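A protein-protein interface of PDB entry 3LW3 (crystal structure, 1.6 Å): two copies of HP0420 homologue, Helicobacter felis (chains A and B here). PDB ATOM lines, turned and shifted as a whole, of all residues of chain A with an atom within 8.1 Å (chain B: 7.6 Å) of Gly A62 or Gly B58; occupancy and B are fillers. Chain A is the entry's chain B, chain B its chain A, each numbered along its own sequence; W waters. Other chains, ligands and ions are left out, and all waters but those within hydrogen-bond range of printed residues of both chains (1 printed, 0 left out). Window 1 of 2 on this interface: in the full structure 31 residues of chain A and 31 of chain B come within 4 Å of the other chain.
The backbone carbonyl oxygen of Gly A58 sits close to the backbone carbonyl oxygen of Gly B58 (3.4 Å).
SG of Cys B27 is in hydrogen-bond range of O of Gly B62 (3.5 Å).
The backbone carbonyl oxygen (O) of Met B48 is in hydrogen-bond range of the backbone NH (N) of His B56, 2.9 Å away.
The backbone carbonyl oxygen of Val B61 is in hydrogen-bond range of the side-chain hydroxyl of Ser B65 (2.8 Å).
SG of Cys A27 lies within hydrogen-bond range of O of Gly A62 (3.6 Å).
The backbone NH (N) of Gly A58 lies close to a ring nitrogen (ND1) of His A56, at 3.4 Å.
The backbone carbonyl oxygen (O) of Val A61 lies within hydrogen-bond range of the side-chain hydroxyl (OG) of Ser A65 (2.9 Å).
Among the printed residues, pairs that only touch across the chains: Leu A22 with His B56, Cys A27 with His B56, His A56 with Cys B27, His A56 with Gly B62, His A56 with Ser B65, Ala A57 with Ser B65, Gly A58 with Gly B62, Gly A62 with His B56, Gly A62 with Gly B58, Ser A65 with His B56, Ser A65 with Ala B57, Phe A66 with His B56 and Ile A79 with Leu B86.
Of chain B, only His B56 and Gly B58 come within 4 Å of Gly A62.
Gly B58 touches just these residues of chain A: Gly A58 (3.4 Å) and Gly A62 (3.4 Å).
Ala B57 touches just one residue of chain A: Ser A65 (3.8 Å).
Of the printed residues of chain B, His A56 touches Cys B27, Gly B62 and Ser B65.
Of the printed residues of chain A, Ser B65 touches His A56 (3.8 Å) and Ala A57 (3.6 Å).
Of the printed residues of chain A, Gly B62 touches His A56 and Gly A58.
Printed residues of chain A within 4 Å of Leu B86: Ile A79 (3.5 Å).
Of the printed residues of chain A, His B56 touches Leu A22 (3.7 Å), Cys A27 (3.8 Å), Gly A62 (3.1 Å), Ser A65 (3.97 Å) and Phe A66 (3.8 Å).
Ala B64 touches none of the printed residues of chain A.
Phe A128 touches none of the printed residues of chain B.
The nearest residue of chain B that does not touch Gly A62 is Ala B57 (5.1 Å).
Printed residues of chain A that touch a printed residue of chain B: Leu A22, Cys A27, His A56, Ala A57, Gly A58, Gly A62, Ser A65, Phe A66 and Ile A79.
Hydrophobic or aromatic side chains of chain A within 4 Å of the printed part of chain B: Leu A22, His A56, Ala A57 and Ile A79.
Along chain A the printed residues that touch a printed residue of chain B span positions 22 to 79.
Hydrophobic or aromatic side chains of chain B within 4 Å of the printed part of chain A: His B56, Ala B57 and Leu B86.
Among the printed residues, 14 pairs touch across the chains.
Cys A27 touches His B56, and with the chains exchanged His A56 touches Cys B27.
Ala A57 touches Ser B65, and with the chains exchanged Ser A65 touches Ala B57.
Gly B58 touches its own counterpart, Gly A58.
Gly A58 touches Gly B62, and with the chains exchanged Gly A62 touches Gly B58.
12 positions are printed for both chains.
Water W1 lies within hydrogen-bond range of the backbone carbonyl oxygen (O) of Gly B58 and the backbone NH (N) of Phe A59.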
ATOM      1  N   CYS A  19     -13.934  -6.609 -20.475  1.00  0.00           N
ATOM      2  CA  CYS A  19     -13.662  -5.808 -21.667  1.00  0.00           C
ATOM      3  C   CYS A  19     -14.426  -6.263 -22.907  1.00  0.00           C
ATOM      4  O   CYS A  19     -13.867  -6.470 -23.976  1.00  0.00           O
ATOM      5  CB  CYS A  19     -12.160  -5.702 -21.945  1.00  0.00           C
ATOM      6  SG  CYS A  19     -11.285  -4.589 -20.723  1.00  0.00           S
ATOM      7  N   LEU A  22     -13.674  -4.215 -26.131  1.00  0.00           N
ATOM      8  CA  LEU A  22     -12.299  -4.035 -26.600  1.00  0.00           C
ATOM      9  C   LEU A  22     -12.006  -4.667 -27.969  1.00  0.00           C
ATOM     10  O   LEU A  22     -12.217  -5.880 -28.198  1.00  0.00           O
ATOM     11  CB  LEU A  22     -11.297  -4.552 -25.558  1.00  0.00           C
ATOM     12  CG  LEU A  22      -9.832  -4.097 -25.727  1.00  0.00           C
ATOM     13  CD1 LEU A  22      -9.645  -2.655 -26.232  1.00  0.00           C
ATOM     14  CD2 LEU A  22      -9.098  -4.215 -24.422  1.00  0.00           C
ATOM     15  N   LEU A  26      -6.578  -3.311 -31.650  1.00  0.00           N
ATOM     16  CA  LEU A  26      -5.969  -2.091 -31.109  1.00  0.00           C
ATOM     17  C   LEU A  26      -5.195  -2.400 -29.822  1.00  0.00           C
ATOM     18  O   LEU A  26      -4.576  -1.494 -29.213  1.00  0.00           O
ATOM     19  CB  LEU A  26      -7.008  -0.995 -30.814  1.00  0.00           C
ATOM     20  CG  LEU A  26      -8.248  -0.773 -31.715  1.00  0.00           C
ATOM     21  CD1 LEU A  26      -8.961   0.564 -31.472  1.00  0.00           C
ATOM     22  CD2 LEU A  26      -7.989  -0.935 -33.148  1.00  0.00           C
ATOM     23  N   CYS A  27      -5.185  -3.668 -29.397  1.00  0.00           N
ATOM     24  CA  CYS A  27      -4.579  -3.973 -28.079  1.00  0.00           C
ATOM     25  C   CYS A  27      -3.570  -5.121 -28.147  1.00  0.00           C
ATOM     26  O   CYS A  27      -2.347  -4.906 -28.150  1.00  0.00           O
ATOM     27  CB  CYS A  27      -5.677  -4.285 -27.071  1.00  0.00           C
ATOM     28  SG  CYS A  27      -5.056  -4.594 -25.407  1.00  0.00           S
ATOM     29  N   ALA A  28      -4.095  -6.338 -28.238  1.00  0.00           N
ATOM     30  CA  ALA A  28      -3.319  -7.576 -28.244  1.00  0.00           C
ATOM     31  C   ALA A  28      -4.306  -8.708 -28.529  1.00  0.00           C
ATOM     32  O   ALA A  28      -5.500  -8.610 -28.258  1.00  0.00           O
ATOM     33  CB  ALA A  28      -2.623  -7.818 -26.889  1.00  0.00           C
ATOM     34  N   VAL A  40      -1.803 -12.862 -23.500  1.00  0.00           N
ATOM     35  CA  VAL A  40      -2.134 -12.184 -24.754  1.00  0.00           C
ATOM     36  C   VAL A  40      -0.850 -11.964 -25.526  1.00  0.00           C
ATOM     37  O   VAL A  40       0.268 -11.925 -24.931  1.00  0.00           O
ATOM     38  CB  VAL A  40      -2.884 -10.853 -24.516  1.00  0.00           C
ATOM     39  CG1 VAL A  40      -4.055 -11.048 -23.535  1.00  0.00           C
ATOM     40  CG2 VAL A  40      -1.942  -9.747 -24.039  1.00  0.00           C
ATOM     41  N   LEU A  42       1.017  -9.343 -28.322  1.00  0.00           N
ATOM     42  CA  LEU A  42       1.057  -8.092 -29.071  1.00  0.00           C
ATOM     43  C   LEU A  42       2.093  -8.159 -30.174  1.00  0.00           C
ATOM     44  O   LEU A  42       3.266  -8.335 -29.908  1.00  0.00           O
ATOM     45  CB  LEU A  42       1.397  -6.931 -28.144  1.00  0.00           C
ATOM     46  CG  LEU A  42       1.657  -5.583 -28.827  1.00  0.00           C
ATOM     47  CD1 LEU A  42       0.421  -5.071 -29.451  1.00  0.00           C
ATOM     48  CD2 LEU A  42       2.233  -4.574 -27.846  1.00  0.00           C
ATOM     49  N   HIS A  56       4.749   3.046 -28.650  1.00  0.00           N
ATOM     50  CA  HIS A  56       4.267   3.899 -27.579  1.00  0.00           C
ATOM     51  C   HIS A  56       3.895   3.149 -26.295  1.00  0.00           C
ATOM     52  O   HIS A  56       3.249   2.065 -26.352  1.00  0.00           O
ATOM     53  CB  HIS A  56       3.036   4.658 -28.031  1.00  0.00           C
ATOM     54  CG  HIS A  56       2.710   5.805 -27.137  1.00  0.00           C
ATOM     55  ND1 HIS A  56       1.479   5.994 -26.567  1.00  0.00           N
ATOM     56  CD2 HIS A  56       3.484   6.829 -26.715  1.00  0.00           C
ATOM     57  CE1 HIS A  56       1.503   7.098 -25.832  1.00  0.00           C
ATOM     58  NE2 HIS A  56       2.703   7.626 -25.925  1.00  0.00           N
ATOM     59  N   ALA A  57       4.303   3.716 -25.154  1.00  0.00           N
ATOM     60  CA  ALA A  57       4.011   3.096 -23.863  1.00  0.00           C
ATOM     61  C   ALA A  57       2.522   2.768 -23.664  1.00  0.00           C
ATOM     62  O   ALA A  57       2.214   1.792 -22.959  1.00  0.00           O
ATOM     63  CB  ALA A  57       4.527   3.960 -22.701  1.00  0.00           C
ATOM     64  N   GLY A  58       1.599   3.557 -24.224  1.00  0.00           N
ATOM     65  CA  GLY A  58       0.186   3.234 -24.096  1.00  0.00           C
ATOM     66  C   GLY A  58      -0.137   1.831 -24.620  1.00  0.00           C
ATOM     67  O   GLY A  58      -0.922   1.111 -23.990  1.00  0.00           O
ATOM     68  N   PHE A  59       0.447   1.435 -25.756  1.00  0.00           N
ATOM     69  CA  PHE A  59       0.212   0.101 -26.303  1.00  0.00           C
ATOM     70  C   PHE A  59       0.904  -1.047 -25.512  1.00  0.00           C
ATOM     71  O   PHE A  59       0.321  -2.129 -25.328  1.00  0.00           O
ATOM     72  CB  PHE A  59       0.474   0.099 -27.808  1.00  0.00           C
ATOM     73  CG  PHE A  59      -0.517   0.974 -28.544  1.00  0.00           C
ATOM     74  CD1 PHE A  59      -1.848   0.535 -28.725  1.00  0.00           C
ATOM     75  CD2 PHE A  59      -0.149   2.218 -29.029  1.00  0.00           C
ATOM     76  CE1 PHE A  59      -2.786   1.330 -29.372  1.00  0.00           C
ATOM     77  CE2 PHE A  59      -1.109   3.023 -29.663  1.00  0.00           C
ATOM     78  CZ  PHE A  59      -2.406   2.591 -29.821  1.00  0.00           C
ATOM     79  N   ILE A  60       2.117  -0.802 -25.018  1.00  0.00           N
ATOM     80  CA  ILE A  60       2.805  -1.818 -24.202  1.00  0.00           C
ATOM     81  C   ILE A  60       2.007  -2.075 -22.896  1.00  0.00           C
ATOM     82  O   ILE A  60       1.585  -3.210 -22.563  1.00  0.00           O
ATOM     83  CB  ILE A  60       4.224  -1.397 -23.873  1.00  0.00           C
ATOM     84  CG1 ILE A  60       5.069  -1.238 -25.151  1.00  0.00           C
ATOM     85  CG2 ILE A  60       4.847  -2.353 -22.827  1.00  0.00           C
ATOM     86  CD1 ILE A  60       4.952  -2.387 -26.116  1.00  0.00           C
ATOM     87  N   VAL A  61       1.721  -0.999 -22.175  1.00  0.00           N
ATOM     88  CA  VAL A  61       0.961  -1.103 -20.934  1.00  0.00           C
ATOM     89  C   VAL A  61      -0.497  -1.554 -21.239  1.00  0.00           C
ATOM     90  O   VAL A  61      -1.071  -2.288 -20.469  1.00  0.00           O
ATOM     91  CB  VAL A  61       1.046   0.191 -20.168  1.00  0.00           C
ATOM     92  CG1 VAL A  61       0.188   0.108 -18.905  1.00  0.00           C
ATOM     93  CG2 VAL A  61       2.544   0.509 -19.882  1.00  0.00           C
ATOM     94  N   GLY A  62      -1.075  -1.104 -22.345  1.00  0.00           N
ATOM     95  CA  GLY A  62      -2.449  -1.458 -22.735  1.00  0.00           C
ATOM     96  C   GLY A  62      -2.558  -2.975 -22.899  1.00  0.00           C
ATOM     97  O   GLY A  62      -3.477  -3.586 -22.381  1.00  0.00           O
ATOM     98  N   ALA A  63      -1.572  -3.592 -23.572  1.00  0.00           N
ATOM     99  CA  ALA A  63      -1.570  -5.057 -23.736  1.00  0.00           C
ATOM    100  C   ALA A  63      -1.468  -5.762 -22.353  1.00  0.00           C
ATOM    101  O   ALA A  63      -2.215  -6.714 -22.064  1.00  0.00           O
ATOM    102  CB  ALA A  63      -0.425  -5.470 -24.638  1.00  0.00           C
ATOM    103  N   ALA A  64      -0.561  -5.263 -21.499  1.00  0.00           N
ATOM    104  CA  ALA A  64      -0.345  -5.831 -20.162  1.00  0.00           C
ATOM    105  C   ALA A  64      -1.640  -5.724 -19.354  1.00  0.00           C
ATOM    106  O   ALA A  64      -2.065  -6.674 -18.668  1.00  0.00           O
ATOM    107  CB  ALA A  64       0.766  -5.103 -19.469  1.00  0.00           C
ATOM    108  N   SER A  65      -2.295  -4.578 -19.467  1.00  0.00           N
ATOM    109  CA  SER A  65      -3.567  -4.289 -18.772  1.00  0.00           C
ATOM    110  C   SER A  65      -4.674  -5.298 -19.135  1.00  0.00           C
ATOM    111  O   SER A  65      -5.357  -5.848 -18.268  1.00  0.00           O
ATOM    112  CB  SER A  65      -4.044  -2.844 -19.078  1.00  0.00           C
ATOM    113  OG  SER A  65      -3.171  -1.870 -18.524  1.00  0.00           O
ATOM    114  N   PHE A  66      -4.830  -5.536 -20.428  1.00  0.00           N
ATOM    115  CA  PHE A  66      -5.760  -6.510 -20.924  1.00  0.00           C
ATOM    116  C   PHE A  66      -5.428  -7.885 -20.378  1.00  0.00           C
ATOM    117  O   PHE A  66      -6.330  -8.555 -19.856  1.00  0.00           O
ATOM    118  CB  PHE A  66      -5.760  -6.477 -22.441  1.00  0.00           C
ATOM    119  CG  PHE A  66      -6.702  -7.447 -23.089  1.00  0.00           C
ATOM    120  CD1 PHE A  66      -8.004  -7.641 -22.619  1.00  0.00           C
ATOM    121  CD2 PHE A  66      -6.311  -8.103 -24.245  1.00  0.00           C
ATOM    122  CE1 PHE A  66      -8.869  -8.534 -23.258  1.00  0.00           C
ATOM    123  CE2 PHE A  66      -7.152  -8.964 -24.909  1.00  0.00           C
ATOM    124  CZ  PHE A  66      -8.441  -9.219 -24.398  1.00  0.00           C
ATOM    125  N   ALA A  67      -4.166  -8.328 -20.467  1.00  0.00           N
ATOM    126  CA  ALA A  67      -3.769  -9.640 -19.851  1.00  0.00           C
ATOM    127  C   ALA A  67      -4.213  -9.714 -18.363  1.00  0.00           C
ATOM    128  O   ALA A  67      -4.815 -10.713 -17.914  1.00  0.00           O
ATOM    129  CB  ALA A  67      -2.260  -9.893 -19.898  1.00  0.00           C
ATOM    130  N   ALA A  68      -3.870  -8.658 -17.621  1.00  0.00           N
ATOM    131  CA  ALA A  68      -4.189  -8.571 -16.180  1.00  0.00           C
ATOM    132  C   ALA A  68      -5.704  -8.762 -15.953  1.00  0.00           C
ATOM    133  O   ALA A  68      -6.111  -9.590 -15.152  1.00  0.00           O
ATOM    134  CB  ALA A  68      -3.715  -7.246 -15.624  1.00  0.00           C
ATOM    135  N   LEU A  69      -6.540  -8.017 -16.677  1.00  0.00           N
ATOM    136  CA  LEU A  69      -8.010  -8.137 -16.548  1.00  0.00           C
ATOM    137  C   LEU A  69      -8.474  -9.559 -16.893  1.00  0.00           C
ATOM    138  O   LEU A  69      -9.324 -10.107 -16.209  1.00  0.00           O
ATOM    139  CB  LEU A  69      -8.716  -7.071 -17.383  1.00  0.00           C
ATOM    140  CG  LEU A  69      -8.596  -5.674 -16.764  1.00  0.00           C
ATOM    141  CD1 LEU A  69      -8.905  -4.463 -17.731  1.00  0.00           C
ATOM    142  CD2 LEU A  69      -9.524  -5.627 -15.543  1.00  0.00           C
ATOM    143  N   ILE A  79      -9.165  -1.657 -13.467  1.00  0.00           N
ATOM    144  CA  ILE A  79      -7.815  -1.416 -12.984  1.00  0.00           C
ATOM    145  C   ILE A  79      -7.774  -0.094 -12.215  1.00  0.00           C
ATOM    146  O   ILE A  79      -8.141   0.965 -12.747  1.00  0.00           O
ATOM    147  CB  ILE A  79      -6.781  -1.382 -14.161  1.00  0.00           C
ATOM    148  CG1 ILE A  79      -6.748  -2.755 -14.880  1.00  0.00           C
ATOM    149  CG2 ILE A  79      -5.429  -0.917 -13.653  1.00  0.00           C
ATOM    150  CD1 ILE A  79      -5.959  -2.715 -16.156  1.00  0.00           C
ATOM    151  N   MET A  82      -1.273   0.705 -11.059  1.00  0.00           N
ATOM    152  CA  MET A  82      -0.235  -0.180 -11.556  1.00  0.00           C
ATOM    153  C   MET A  82       1.138   0.389 -11.297  1.00  0.00           C
ATOM    154  O   MET A  82       1.314   1.603 -11.186  1.00  0.00           O
ATOM    155  CB  MET A  82      -0.409  -0.373 -13.073  1.00  0.00           C
ATOM    156  CG  MET A  82      -0.105   0.886 -13.885  1.00  0.00           C
ATOM    157  SD  MET A  82      -0.551   0.739 -15.641  1.00  0.00           S
ATOM    158  CE  MET A  82      -2.316   0.594 -15.612  1.00  0.00           C
ATOM    159  N   PHE A  98       2.435 -11.424 -23.226  1.00  0.00           N
ATOM    160  CA  PHE A  98       2.216 -10.966 -21.859  1.00  0.00           C
ATOM    161  C   PHE A  98       1.488 -12.029 -21.070  1.00  0.00           C
ATOM    162  O   PHE A  98       0.352 -12.388 -21.403  1.00  0.00           O
ATOM    163  CB  PHE A  98       1.387  -9.682 -21.817  1.00  0.00           C
ATOM    164  CG  PHE A  98       2.099  -8.492 -22.450  1.00  0.00           C
ATOM    165  CD1 PHE A  98       2.844  -7.597 -21.667  1.00  0.00           C
ATOM    166  CD2 PHE A  98       2.031  -8.271 -23.824  1.00  0.00           C
ATOM    167  CE1 PHE A  98       3.478  -6.516 -22.252  1.00  0.00           C
ATOM    168  CE2 PHE A  98       2.713  -7.143 -24.403  1.00  0.00           C
ATOM    169  CZ  PHE A  98       3.386  -6.285 -23.604  1.00  0.00           C
ATOM    170  N   PHE A 124       9.243  -6.691 -20.156  1.00  0.00           N
ATOM    171  CA  PHE A 124       8.245  -5.906 -19.419  1.00  0.00           C
ATOM    172  C   PHE A 124       7.927  -6.633 -18.124  1.00  0.00           C
ATOM    173  O   PHE A 124       7.823  -7.867 -18.088  1.00  0.00           O
ATOM    174  CB  PHE A 124       6.965  -5.777 -20.263  1.00  0.00           C
ATOM    175  CG  PHE A 124       5.834  -5.091 -19.551  1.00  0.00           C
ATOM    176  CD1 PHE A 124       5.697  -3.695 -19.626  1.00  0.00           C
ATOM    177  CD2 PHE A 124       4.938  -5.819 -18.770  1.00  0.00           C
ATOM    178  CE1 PHE A 124       4.680  -3.044 -18.947  1.00  0.00           C
ATOM    179  CE2 PHE A 124       3.909  -5.169 -18.093  1.00  0.00           C
ATOM    180  CZ  PHE A 124       3.767  -3.791 -18.204  1.00  0.00           C
ATOM    181  N   PHE A 128      -0.518  -5.024 -11.289  1.00  0.00           N
ATOM    182  CA  PHE A 128      -1.756  -4.278 -11.500  1.00  0.00           C
ATOM    183  C   PHE A 128      -2.681  -4.540 -10.313  1.00  0.00           C
ATOM    184  O   PHE A 128      -2.779  -5.670  -9.848  1.00  0.00           O
ATOM    185  CB  PHE A 128      -2.456  -4.739 -12.782  1.00  0.00           C
ATOM    186  CG  PHE A 128      -1.657  -4.437 -14.020  1.00  0.00           C
ATOM    187  CD1 PHE A 128      -1.955  -3.335 -14.785  1.00  0.00           C
ATOM    188  CD2 PHE A 128      -0.544  -5.231 -14.350  1.00  0.00           C
ATOM    189  CE1 PHE A 128      -1.168  -3.021 -15.896  1.00  0.00           C
ATOM    190  CE2 PHE A 128       0.233  -4.942 -15.448  1.00  0.00           C
ATOM    191  CZ  PHE A 128      -0.058  -3.811 -16.203  1.00  0.00           C
ATOM    192  N   LEU B  26      -5.299   8.812 -32.226  1.00  0.00           N
ATOM    193  CA  LEU B  26      -5.381   7.593 -31.432  1.00  0.00           C
ATOM    194  C   LEU B  26      -4.929   7.782 -29.992  1.00  0.00           C
ATOM    195  O   LEU B  26      -5.019   6.844 -29.208  1.00  0.00           O
ATOM    196  CB  LEU B  26      -4.561   6.476 -32.081  1.00  0.00           C
ATOM    197  CG  LEU B  26      -5.038   6.097 -33.484  1.00  0.00           C
ATOM    198  CD1 LEU B  26      -4.188   4.958 -34.051  1.00  0.00           C
ATOM    199  CD2 LEU B  26      -6.527   5.708 -33.511  1.00  0.00           C
ATOM    200  N   CYS B  27      -4.469   8.988 -29.628  1.00  0.00           N
ATOM    201  CA  CYS B  27      -3.841   9.212 -28.317  1.00  0.00           C
ATOM    202  C   CYS B  27      -4.460  10.427 -27.644  1.00  0.00           C
ATOM    203  O   CYS B  27      -5.328  10.288 -26.834  1.00  0.00           O
ATOM    204  CB  CYS B  27      -2.318   9.374 -28.469  1.00  0.00           C
ATOM    205  SG  CYS B  27      -1.399   9.614 -26.936  1.00  0.00           S
ATOM    206  N   MET B  48     -11.723   3.212 -28.221  1.00  0.00           N
ATOM    207  CA  MET B  48     -10.858   3.178 -27.034  1.00  0.00           C
ATOM    208  C   MET B  48     -11.485   2.428 -25.882  1.00  0.00           C
ATOM    209  O   MET B  48     -10.865   2.270 -24.832  1.00  0.00           O
ATOM    210  CB  MET B  48     -10.515   4.596 -26.554  1.00  0.00           C
ATOM    211  CG  MET B  48      -9.725   5.414 -27.537  1.00  0.00           C
ATOM    212  SD  MET B  48      -9.428   7.047 -26.831  1.00  0.00           S
ATOM    213  CE  MET B  48      -8.282   7.749 -27.975  1.00  0.00           C
ATOM    214  N   VAL B  55     -13.154   3.500 -20.548  1.00  0.00           N
ATOM    215  CA  VAL B  55     -12.102   3.608 -21.533  1.00  0.00           C
ATOM    216  C   VAL B  55     -10.962   2.661 -21.081  1.00  0.00           C
ATOM    217  O   VAL B  55     -10.623   2.595 -19.887  1.00  0.00           O
ATOM    218  CB  VAL B  55     -11.606   5.067 -21.656  1.00  0.00           C
ATOM    219  CG1 VAL B  55     -10.330   5.095 -22.418  1.00  0.00           C
ATOM    220  CG2 VAL B  55     -12.652   5.985 -22.326  1.00  0.00           C
ATOM    221  N   HIS B  56     -10.375   1.950 -22.032  1.00  0.00           N
ATOM    222  CA  HIS B  56      -9.325   1.011 -21.705  1.00  0.00           C
ATOM    223  C   HIS B  56      -8.147   1.734 -21.104  1.00  0.00           C
ATOM    224  O   HIS B  56      -7.747   2.801 -21.598  1.00  0.00           O
ATOM    225  CB  HIS B  56      -8.863   0.259 -22.956  1.00  0.00           C
ATOM    226  CG  HIS B  56      -7.906  -0.847 -22.641  1.00  0.00           C
ATOM    227  ND1 HIS B  56      -6.709  -1.014 -23.292  1.00  0.00           N
ATOM    228  CD2 HIS B  56      -7.994  -1.856 -21.744  1.00  0.00           C
ATOM    229  CE1 HIS B  56      -6.106  -2.088 -22.821  1.00  0.00           C
ATOM    230  NE2 HIS B  56      -6.856  -2.607 -21.866  1.00  0.00           N
ATOM    231  N   ALA B  57      -7.547   1.136 -20.079  1.00  0.00           N
ATOM    232  CA  ALA B  57      -6.379   1.715 -19.409  1.00  0.00           C
ATOM    233  C   ALA B  57      -5.214   2.075 -20.351  1.00  0.00           C
ATOM    234  O   ALA B  57      -4.470   3.044 -20.099  1.00  0.00           O
ATOM    235  CB  ALA B  57      -5.927   0.793 -18.282  1.00  0.00           C
ATOM    236  N   GLY B  58      -5.032   1.314 -21.428  1.00  0.00           N
ATOM    237  CA  GLY B  58      -3.963   1.603 -22.383  1.00  0.00           C
ATOM    238  C   GLY B  58      -4.075   3.006 -22.985  1.00  0.00           C
ATOM    239  O   GLY B  58      -3.054   3.690 -23.167  1.00  0.00           O
ATOM    240  N   PHE B  59      -5.302   3.474 -23.265  1.00  0.00           N
ATOM    241  CA  PHE B  59      -5.476   4.818 -23.834  1.00  0.00           C
ATOM    242  C   PHE B  59      -5.299   5.946 -22.806  1.00  0.00           C
ATOM    243  O   PHE B  59      -4.808   7.030 -23.121  1.00  0.00           O
ATOM    244  CB  PHE B  59      -6.809   4.905 -24.566  1.00  0.00           C
ATOM    245  CG  PHE B  59      -6.819   4.079 -25.821  1.00  0.00           C
ATOM    246  CD1 PHE B  59      -6.190   4.554 -26.978  1.00  0.00           C
ATOM    247  CD2 PHE B  59      -7.428   2.827 -25.840  1.00  0.00           C
ATOM    248  CE1 PHE B  59      -6.184   3.793 -28.146  1.00  0.00           C
ATOM    249  CE2 PHE B  59      -7.430   2.071 -27.020  1.00  0.00           C
ATOM    250  CZ  PHE B  59      -6.777   2.556 -28.152  1.00  0.00           C
ATOM    251  N   ILE B  60      -5.650   5.663 -21.569  1.00  0.00           N
ATOM    252  CA  ILE B  60      -5.476   6.637 -20.482  1.00  0.00           C
ATOM    253  C   ILE B  60      -3.974   6.794 -20.192  1.00  0.00           C
ATOM    254  O   ILE B  60      -3.427   7.898 -20.170  1.00  0.00           O
ATOM    255  CB  ILE B  60      -6.220   6.197 -19.216  1.00  0.00           C
ATOM    256  CG1 ILE B  60      -7.745   6.203 -19.504  1.00  0.00           C
ATOM    257  CG2 ILE B  60      -5.855   7.114 -18.082  1.00  0.00           C
ATOM    258  CD1 ILE B  60      -8.555   5.532 -18.505  1.00  0.00           C
ATOM    259  N   VAL B  61      -3.298   5.662 -19.946  1.00  0.00           N
ATOM    260  CA  VAL B  61      -1.845   5.654 -19.814  1.00  0.00           C
ATOM    261  C   VAL B  61      -1.133   6.218 -21.056  1.00  0.00           C
ATOM    262  O   VAL B  61      -0.155   6.932 -20.904  1.00  0.00           O
ATOM    263  CB  VAL B  61      -1.327   4.250 -19.492  1.00  0.00           C
ATOM    264  CG1 VAL B  61       0.227   4.209 -19.562  1.00  0.00           C
ATOM    265  CG2 VAL B  61      -1.843   3.828 -18.101  1.00  0.00           C
ATOM    266  N   GLY B  62      -1.609   5.890 -22.259  1.00  0.00           N
ATOM    267  CA  GLY B  62      -1.034   6.385 -23.505  1.00  0.00           C
ATOM    268  C   GLY B  62      -1.068   7.918 -23.531  1.00  0.00           C
ATOM    269  O   GLY B  62      -0.060   8.557 -23.839  1.00  0.00           O
ATOM    270  N   ALA B  63      -2.217   8.507 -23.151  1.00  0.00           N
ATOM    271  CA  ALA B  63      -2.368   9.966 -23.149  1.00  0.00           C
ATOM    272  C   ALA B  63      -1.406  10.574 -22.147  1.00  0.00           C
ATOM    273  O   ALA B  63      -0.677  11.530 -22.471  1.00  0.00           O
ATOM    274  CB  ALA B  63      -3.771  10.374 -22.841  1.00  0.00           C
ATOM    275  N   ALA B  64      -1.382  10.038 -20.920  1.00  0.00           N
ATOM    276  CA  ALA B  64      -0.459  10.537 -19.876  1.00  0.00           C
ATOM    277  C   ALA B  64       1.015  10.424 -20.294  1.00  0.00           C
ATOM    278  O   ALA B  64       1.849  11.314 -20.054  1.00  0.00           O
ATOM    279  CB  ALA B  64      -0.709   9.799 -18.527  1.00  0.00           C
ATOM    280  N   SER B  65       1.345   9.297 -20.915  1.00  0.00           N
ATOM    281  CA  SER B  65       2.686   9.015 -21.410  1.00  0.00           C
ATOM    282  C   SER B  65       3.140  10.071 -22.407  1.00  0.00           C
ATOM    283  O   SER B  65       4.290  10.559 -22.344  1.00  0.00           O
ATOM    284  CB  SER B  65       2.728   7.619 -22.081  1.00  0.00           C
ATOM    285  OG  SER B  65       2.606   6.575 -21.082  1.00  0.00           O
ATOM    286  N   LEU B  86      -5.387   5.075 -11.360  1.00  0.00           N
ATOM    287  CA  LEU B  86      -6.552   5.426 -12.181  1.00  0.00           C
ATOM    288  C   LEU B  86      -7.655   5.688 -11.169  1.00  0.00           C
ATOM    289  O   LEU B  86      -8.130   4.754 -10.485  1.00  0.00           O
ATOM    290  CB  LEU B  86      -6.917   4.261 -13.117  1.00  0.00           C
ATOM    291  CG  LEU B  86      -5.776   3.804 -14.052  1.00  0.00           C
ATOM    292  CD1 LEU B  86      -6.243   2.726 -15.053  1.00  0.00           C
ATOM    293  CD2 LEU B  86      -5.303   4.961 -14.777  1.00  0.00           C
HETATM  294  O   HOH W   1      -2.255   3.444 -26.487  1.00  0.00           O
